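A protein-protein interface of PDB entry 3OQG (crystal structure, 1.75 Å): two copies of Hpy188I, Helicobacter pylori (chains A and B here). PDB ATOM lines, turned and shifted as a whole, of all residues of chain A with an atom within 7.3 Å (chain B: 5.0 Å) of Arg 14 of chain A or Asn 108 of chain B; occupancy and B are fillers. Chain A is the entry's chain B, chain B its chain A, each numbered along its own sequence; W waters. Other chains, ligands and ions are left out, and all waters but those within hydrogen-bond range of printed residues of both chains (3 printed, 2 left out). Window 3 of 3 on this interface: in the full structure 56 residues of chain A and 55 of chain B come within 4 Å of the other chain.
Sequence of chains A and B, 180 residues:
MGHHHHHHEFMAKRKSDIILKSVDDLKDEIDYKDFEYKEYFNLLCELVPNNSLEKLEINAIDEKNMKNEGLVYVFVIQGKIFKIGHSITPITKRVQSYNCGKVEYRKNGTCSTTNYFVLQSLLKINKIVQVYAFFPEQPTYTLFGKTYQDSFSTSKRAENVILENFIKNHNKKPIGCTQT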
ATOM      1  N   PHE A  10      21.939 -13.838 -30.004  1.00  0.00           N
ATOM      2  CA  PHE A  10      21.614 -14.785 -28.933  1.00  0.00           C
ATOM      3  C   PHE A  10      21.496 -16.206 -29.499  1.00  0.00           C
ATOM      4  O   PHE A  10      21.154 -16.380 -30.682  1.00  0.00           O
ATOM      5  CB  PHE A  10      20.295 -14.384 -28.251  1.00  0.00           C
ATOM      6  CG  PHE A  10      19.107 -14.407 -29.175  1.00  0.00           C
ATOM      7  CD1 PHE A  10      18.331 -15.555 -29.301  1.00  0.00           C
ATOM      8  CD2 PHE A  10      18.772 -13.285 -29.933  1.00  0.00           C
ATOM      9  CE1 PHE A  10      17.240 -15.585 -30.167  1.00  0.00           C
ATOM     10  CE2 PHE A  10      17.689 -13.309 -30.805  1.00  0.00           C
ATOM     11  CZ  PHE A  10      16.920 -14.460 -30.918  1.00  0.00           C
ATOM     12  N   MET A  11      21.786 -17.213 -28.665  1.00  0.00           N
ATOM     13  CA  MET A  11      21.491 -18.611 -29.015  1.00  0.00           C
ATOM     14  C   MET A  11      19.996 -18.871 -28.767  1.00  0.00           C
ATOM     15  O   MET A  11      19.550 -19.005 -27.616  1.00  0.00           O
ATOM     16  CB  MET A  11      22.321 -19.620 -28.194  1.00  0.00           C
ATOM     17  CG  MET A  11      23.858 -19.639 -28.408  1.00  0.00           C
ATOM     18  SD  MET A  11      24.481 -19.227 -30.059  1.00  0.00           S
ATOM     19  CE  MET A  11      24.635 -17.460 -29.827  1.00  0.00           C
ATOM     20  N   ALA A  12      19.222 -18.913 -29.851  1.00  0.00           N
ATOM     21  CA  ALA A  12      17.820 -19.298 -29.776  1.00  0.00           C
ATOM     22  C   ALA A  12      17.706 -20.739 -29.274  1.00  0.00           C
ATOM     23  O   ALA A  12      18.584 -21.585 -29.547  1.00  0.00           O
ATOM     24  CB  ALA A  12      17.162 -19.167 -31.150  1.00  0.00           C
ATOM     25  N   LYS A  13      16.633 -21.023 -28.546  1.00  0.00           N
ATOM     26  CA  LYS A  13      16.348 -22.384 -28.113  1.00  0.00           C
ATOM     27  C   LYS A  13      15.369 -23.072 -29.061  1.00  0.00           C
ATOM     28  O   LYS A  13      15.131 -24.278 -28.945  1.00  0.00           O
ATOM     29  CB  LYS A  13      15.786 -22.370 -26.696  1.00  0.00           C
ATOM     30  CG  LYS A  13      16.748 -21.808 -25.671  1.00  0.00           C
ATOM     31  CD  LYS A  13      16.236 -22.029 -24.252  1.00  0.00           C
ATOM     32  CE  LYS A  13      17.281 -21.658 -23.203  1.00  0.00           C
ATOM     33  NZ  LYS A  13      18.595 -22.329 -23.433  1.00  0.00           N
ATOM     34  N   ARG A  14      14.806 -22.301 -29.992  1.00  0.00           N
ATOM     35  CA  ARG A  14      13.758 -22.782 -30.888  1.00  0.00           C
ATOM     36  C   ARG A  14      13.573 -21.773 -32.013  1.00  0.00           C
ATOM     37  O   ARG A  14      13.932 -20.602 -31.868  1.00  0.00           O
ATOM     38  CB  ARG A  14      12.448 -22.942 -30.113  1.00  0.00           C
ATOM     39  CG  ARG A  14      11.995 -21.652 -29.435  1.00  0.00           C
ATOM     40  CD  ARG A  14      10.987 -21.895 -28.335  1.00  0.00           C
ATOM     41  NE  ARG A  14      11.590 -22.494 -27.135  1.00  0.00           N
ATOM     42  CZ  ARG A  14      12.022 -21.817 -26.066  1.00  0.00           C
ATOM     43  NH1 ARG A  14      12.498 -22.459 -25.014  1.00  0.00           N
ATOM     44  NH2 ARG A  14      11.948 -20.492 -26.018  1.00  0.00           N
ATOM     45  N   LYS A  15      12.994 -22.223 -33.123  1.00  0.00           N
ATOM     46  CA  LYS A  15      12.830 -21.382 -34.302  1.00  0.00           C
ATOM     47  C   LYS A  15      12.010 -20.122 -34.017  1.00  0.00           C
ATOM     48  O   LYS A  15      12.355 -19.034 -34.479  1.00  0.00           O
ATOM     49  CB  LYS A  15      12.184 -22.166 -35.456  1.00  0.00           C
ATOM     50  CG  LYS A  15      12.062 -21.334 -36.734  1.00  0.00           C
ATOM     51  CD  LYS A  15      12.264 -22.140 -38.016  1.00  0.00           C
ATOM     52  CE  LYS A  15      10.979 -22.715 -38.552  1.00  0.00           C
ATOM     53  NZ  LYS A  15      11.128 -23.215 -39.938  1.00  0.00           N
ATOM     54  N   SER A  16      10.939 -20.278 -33.243  1.00  0.00           N
ATOM     55  CA  SER A  16      10.026 -19.166 -32.950  1.00  0.00           C
ATOM     56  C   SER A  16      10.681 -18.003 -32.216  1.00  0.00           C
ATOM     57  O   SER A  16      10.138 -16.885 -32.234  1.00  0.00           O
ATOM     58  CB  SER A  16       8.841 -19.677 -32.133  1.00  0.00           C
ATOM     59  OG  SER A  16       9.267 -20.146 -30.867  1.00  0.00           O
ATOM     60  N   ASP A  17      11.816 -18.270 -31.552  1.00  0.00           N
ATOM     61  CA  ASP A  17      12.592 -17.247 -30.849  1.00  0.00           C
ATOM     62  C   ASP A  17      13.221 -16.257 -31.819  1.00  0.00           C
ATOM     63  O   ASP A  17      13.570 -15.142 -31.410  1.00  0.00           O
ATOM     64  CB  ASP A  17      13.768 -17.824 -30.051  1.00  0.00           C
ATOM     65  CG  ASP A  17      13.357 -18.598 -28.794  1.00  0.00           C
ATOM     66  OD1 ASP A  17      12.186 -18.592 -28.395  1.00  0.00           O
ATOM     67  OD2 ASP A  17      14.263 -19.239 -28.205  1.00  0.00           O
ATOM     68  N   ILE A  18      13.434 -16.681 -33.062  1.00  0.00           N
ATOM     69  CA  ILE A  18      14.166 -15.869 -34.023  1.00  0.00           C
ATOM     70  C   ILE A  18      13.221 -15.042 -34.875  1.00  0.00           C
ATOM     71  O   ILE A  18      12.583 -15.543 -35.804  1.00  0.00           O
ATOM     72  CB  ILE A  18      15.049 -16.731 -34.921  1.00  0.00           C
ATOM     73  CG1 ILE A  18      15.971 -17.580 -34.051  1.00  0.00           C
ATOM     74  CG2 ILE A  18      15.840 -15.829 -35.871  1.00  0.00           C
ATOM     75  CD1 ILE A  18      16.694 -18.683 -34.793  1.00  0.00           C
ATOM     76  N   ARG A 106       4.302 -13.277 -24.412  1.00  0.00           N
ATOM     77  CA  ARG A 106       5.348 -14.277 -24.592  1.00  0.00           C
ATOM     78  C   ARG A 106       6.140 -14.508 -23.309  1.00  0.00           C
ATOM     79  O   ARG A 106       6.446 -15.659 -22.950  1.00  0.00           O
ATOM     80  CB  ARG A 106       6.276 -13.932 -25.766  1.00  0.00           C
ATOM     81  CG  ARG A 106       7.338 -14.999 -26.066  1.00  0.00           C
ATOM     82  CD  ARG A 106       6.737 -16.313 -26.565  1.00  0.00           C
ATOM     83  NE  ARG A 106       7.696 -17.403 -26.655  1.00  0.00           N
ATOM     84  CZ  ARG A 106       8.137 -18.129 -25.629  1.00  0.00           C
ATOM     85  NH1 ARG A 106       7.710 -17.874 -24.398  1.00  0.00           N
ATOM     86  NH2 ARG A 106       9.015 -19.129 -25.843  1.00  0.00           N
ATOM     87  N   LYS A 107       6.451 -13.425 -22.603  1.00  0.00           N
ATOM     88  CA  LYS A 107       7.078 -13.521 -21.280  1.00  0.00           C
ATOM     89  C   LYS A 107       6.176 -14.250 -20.292  1.00  0.00           C
ATOM     90  O   LYS A 107       6.658 -15.060 -19.510  1.00  0.00           O
ATOM     91  CB  LYS A 107       7.414 -12.142 -20.718  1.00  0.00           C
ATOM     92  CG  LYS A 107       8.561 -11.442 -21.397  1.00  0.00           C
ATOM     93  CD  LYS A 107       9.000 -10.197 -20.619  1.00  0.00           C
ATOM     94  CE  LYS A 107       9.966  -9.352 -21.437  1.00  0.00           C
ATOM     95  NZ  LYS A 107      10.922 -10.212 -22.177  1.00  0.00           N
ATOM     96  N   ASN A 108       4.878 -13.931 -20.319  1.00  0.00           N
ATOM     97  CA  ASN A 108       3.878 -14.588 -19.467  1.00  0.00           C
ATOM     98  C   ASN A 108       3.777 -16.098 -19.783  1.00  0.00           C
ATOM     99  O   ASN A 108       3.348 -16.879 -18.931  1.00  0.00           O
ATOM    100  CB  ASN A 108       2.460 -13.956 -19.632  1.00  0.00           C
ATOM    101  CG  ASN A 108       2.329 -12.500 -19.091  1.00  0.00           C
ATOM    102  OD1 ASN A 108       3.241 -11.958 -18.439  1.00  0.00           O
ATOM    103  ND2 ASN A 108       1.155 -11.854 -19.386  1.00  0.00           N
ATOM    104  N   GLY A 109       4.140 -16.488 -21.008  1.00  0.00           N
ATOM    105  CA  GLY A 109       3.877 -17.822 -21.540  1.00  0.00           C
ATOM    106  C   GLY A 109       2.428 -18.078 -21.922  1.00  0.00           C
ATOM    107  O   GLY A 109       1.998 -19.220 -21.979  1.00  0.00           O
ATOM    108  N   THR A 113       3.656 -19.565 -29.409  1.00  0.00           N
ATOM    109  CA  THR A 113       4.926 -19.160 -30.012  1.00  0.00           C
ATOM    110  C   THR A 113       4.735 -18.672 -31.467  1.00  0.00           C
ATOM    111  O   THR A 113       5.404 -17.737 -31.888  1.00  0.00           O
ATOM    112  CB  THR A 113       6.002 -20.254 -29.912  1.00  0.00           C
ATOM    113  OG1 THR A 113       5.611 -21.381 -30.697  1.00  0.00           O
ATOM    114  CG2 THR A 113       6.236 -20.656 -28.447  1.00  0.00           C
ATOM    115  N   GLU B 104       8.722 -27.161 -16.660  1.00  0.00           N
ATOM    116  CA  GLU B 104       9.785 -26.567 -17.468  1.00  0.00           C
ATOM    117  C   GLU B 104       9.269 -25.852 -18.721  1.00  0.00           C
ATOM    118  O   GLU B 104       9.701 -24.740 -19.032  1.00  0.00           O
ATOM    119  CB  GLU B 104      10.831 -27.616 -17.874  1.00  0.00           C
ATOM    120  CG  GLU B 104      12.047 -27.018 -18.595  1.00  0.00           C
ATOM    121  CD  GLU B 104      13.079 -28.047 -19.008  1.00  0.00           C
ATOM    122  OE1 GLU B 104      12.924 -29.249 -18.699  1.00  0.00           O
ATOM    123  OE2 GLU B 104      14.067 -27.639 -19.649  1.00  0.00           O
ATOM    124  N   TYR B 105       8.346 -26.492 -19.435  1.00  0.00           N
ATOM    125  CA  TYR B 105       7.835 -25.927 -20.689  1.00  0.00           C
ATOM    126  C   TYR B 105       6.910 -24.750 -20.395  1.00  0.00           C
ATOM    127  O   TYR B 105       6.914 -23.796 -21.140  1.00  0.00           O
ATOM    128  CB  TYR B 105       7.147 -26.979 -21.564  1.00  0.00           C
ATOM    129  CG  TYR B 105       7.925 -28.275 -21.706  1.00  0.00           C
ATOM    130  CD1 TYR B 105       9.298 -28.316 -21.542  1.00  0.00           C
ATOM    131  CD2 TYR B 105       7.254 -29.453 -21.996  1.00  0.00           C
ATOM    132  CE1 TYR B 105      10.009 -29.551 -21.641  1.00  0.00           C
ATOM    133  CE2 TYR B 105       7.928 -30.675 -22.098  1.00  0.00           C
ATOM    134  CZ  TYR B 105       9.289 -30.715 -21.925  1.00  0.00           C
ATOM    135  OH  TYR B 105       9.934 -31.939 -22.020  1.00  0.00           O
ATOM    136  N   ARG B 106       6.177 -24.804 -19.283  1.00  0.00           N
ATOM    137  CA  ARG B 106       5.362 -23.650 -18.852  1.00  0.00           C
ATOM    138  C   ARG B 106       6.255 -22.462 -18.565  1.00  0.00           C
ATOM    139  O   ARG B 106       5.948 -21.329 -18.962  1.00  0.00           O
ATOM    140  CB  ARG B 106       4.519 -23.981 -17.621  1.00  0.00           C
ATOM    141  CG  ARG B 106       3.557 -22.858 -17.165  1.00  0.00           C
ATOM    142  CD  ARG B 106       2.552 -22.490 -18.241  1.00  0.00           C
ATOM    143  NE  ARG B 106       1.777 -21.291 -17.909  1.00  0.00           N
ATOM    144  CZ  ARG B 106       2.187 -20.046 -18.126  1.00  0.00           C
ATOM    145  NH1 ARG B 106       3.377 -19.819 -18.660  1.00  0.00           N
ATOM    146  NH2 ARG B 106       1.399 -19.010 -17.820  1.00  0.00           N
ATOM    147  N   LYS B 107       7.371 -22.721 -17.896  1.00  0.00           N
ATOM    148  CA  LYS B 107       8.381 -21.687 -17.642  1.00  0.00           C
ATOM    149  C   LYS B 107       9.001 -21.139 -18.929  1.00  0.00           C
ATOM    150  O   LYS B 107       9.209 -19.931 -19.042  1.00  0.00           O
ATOM    151  CB  LYS B 107       9.471 -22.215 -16.714  1.00  0.00           C
ATOM    152  CG  LYS B 107       9.116 -22.099 -15.241  1.00  0.00           C
ATOM    153  CD  LYS B 107      10.267 -22.557 -14.357  1.00  0.00           C
ATOM    154  CE  LYS B 107       9.805 -22.958 -12.963  1.00  0.00           C
ATOM    155  NZ  LYS B 107      10.673 -24.061 -12.420  1.00  0.00           N
ATOM    156  N   ASN B 108       9.281 -22.024 -19.886  1.00  0.00           N
ATOM    157  CA  ASN B 108       9.761 -21.634 -21.222  1.00  0.00           C
ATOM    158  C   ASN B 108       8.677 -20.859 -22.021  1.00  0.00           C
ATOM    159  O   ASN B 108       9.005 -20.130 -22.961  1.00  0.00           O
ATOM    160  CB  ASN B 108      10.165 -22.851 -22.101  1.00  0.00           C
ATOM    161  CG  ASN B 108      11.281 -23.763 -21.503  1.00  0.00           C
ATOM    162  OD1 ASN B 108      12.044 -23.386 -20.602  1.00  0.00           O
ATOM    163  ND2 ASN B 108      11.382 -24.992 -22.070  1.00  0.00           N
ATOM    164  N   GLY B 109       7.403 -21.045 -21.663  1.00  0.00           N
ATOM    165  CA  GLY B 109       6.271 -20.500 -22.419  1.00  0.00           C
ATOM    166  C   GLY B 109       5.965 -21.266 -23.693  1.00  0.00           C
ATOM    167  O   GLY B 109       5.368 -20.722 -24.640  1.00  0.00           O
ATOM    168  N   THR B 110       6.386 -22.532 -23.752  1.00  0.00           N
ATOM    169  CA  THR B 110       6.254 -23.299 -24.972  1.00  0.00           C
ATOM    170  C   THR B 110       5.124 -24.327 -24.977  1.00  0.00           C
ATOM    171  O   THR B 110       4.828 -24.888 -26.032  1.00  0.00           O
ATOM    172  CB  THR B 110       7.574 -24.026 -25.315  1.00  0.00           C
ATOM    173  OG1 THR B 110       7.946 -24.868 -24.214  1.00  0.00           O
ATOM    174  CG2 THR B 110       8.685 -23.003 -25.599  1.00  0.00           C
HETATM  175  O   HOH W   1      11.842 -19.328 -23.157  1.00  0.00           O
HETATM  176  O   HOH W   2       3.302 -21.633 -21.469  1.00  0.00           O
HETATM  177  O   HOH W   3       4.345 -18.076 -24.797  1.00  0.00           O
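O of Asn 108 of chain A lies within hydrogen-bond range of NH1 of Arg 106 of chain B. The guanidinium group (NH1) of Arg 106 of chain A sits at hydrogen-bond distance from the backbone carbonyl oxygen (O) of Asn 108 of chain B, at 3.0 Å.
O of Glu 104 of chain B lies close to OD1 of Asn 108 of chain B (3.1 Å). The backbone NH (N) of Thr 110 of chain B sits at hydrogen-bond distance from the backbone carbonyl oxygen (O) of Tyr 105 of chain B (2.9 Å). The side-chain carboxylate (OD1) of Asp 17 of chain A is in salt-bridge range of the guanidinium group (NH2) of Arg 14 of chain A (3.1 Å).
Among the printed residues, merely in contact across the chains: Arg 14 of chain A with Asn 108 of chain B (3.8 Å), Arg 14 of chain A with Thr 110 of chain B (3.3 Å), Arg 106 of chain A with Gly 109 of chain B (3.6 Å), Arg 106 of chain A with Thr 110 of chain B (3.9 Å), Gly 109 of chain A with Arg 106 of chain B (3.5 Å), Gly 109 of chain A with Gly 109 of chain B (3.7 Å) and Thr 113 of chain A with Gly 109 of chain B (3.9 Å).
Of the printed residues of chain B, Arg 14 of chain A touches Asn 108 (3.8 Å) and Thr 110 (3.3 Å). Of the printed residues of chain A, Asn 108 of chain B touches Arg 14 (3.8 Å) and Arg 106 (3.0 Å). Printed residues of chain B within 4 Å of Gly 109 of chain A: Arg 106 (3.5 Å) and Gly 109 (3.7 Å). Of the printed residues of chain B, Thr 113 of chain A touches Gly 109 (3.9 Å). Printed residues of chain B within 4 Å of Arg 106 of chain A: Asn 108 (3.0 Å), Gly 109 (3.6 Å) and Thr 110 (3.9 Å). Phe 10 of chain A touches none of the printed residues of chain B. The nearest printed residue of chain B that does not touch Arg 14 of chain A is Gly 109 of chain B (6.3 Å).
Of the 14 printed residues of chain A, 5 touch a printed residue of chain B. Printed residues of chain A that touch a printed residue of chain B: Arg 14, Arg 106, Asn 108, Gly 109 and Thr 113. Among the printed residues, no Asp or Glu carboxylate lies within 4 Å of a Lys or Arg side-chain nitrogen of the other chain.
Arg 106 of chain A touches Asn 108 of chain B, and with the chains exchanged Asn 108 of chain A touches Arg 106 of chain B. Arg 106 of chain A touches Gly 109 of chain B, and with the chains exchanged Gly 109 of chain A touches Arg 106 of chain B. Gly 109 of chain B touches its own counterpart, Gly 109 of chain A. 4 positions are printed for both chains. Of the 9 pairs that touch across the chains among the printed residues, 5 have their exchanged pair printed and touching as well.
Water W2 bridges O of Gly 109 of chain A (2.8 Å) and NH1 of Arg 106 of chain B (3.3 Å). Water W3 lies within hydrogen-bond range of the backbone carbonyl oxygen (O) of Gly 109 of chain B (2.8 Å) and the guanidinium group (NH1) of Arg 106 of chain A (3.4 Å). Water W1 bridges the backbone carbonyl oxygen of Asn 108 of chain B (3.0 Å) and the guanidinium group of Arg 14 of chain A (3.1 Å).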
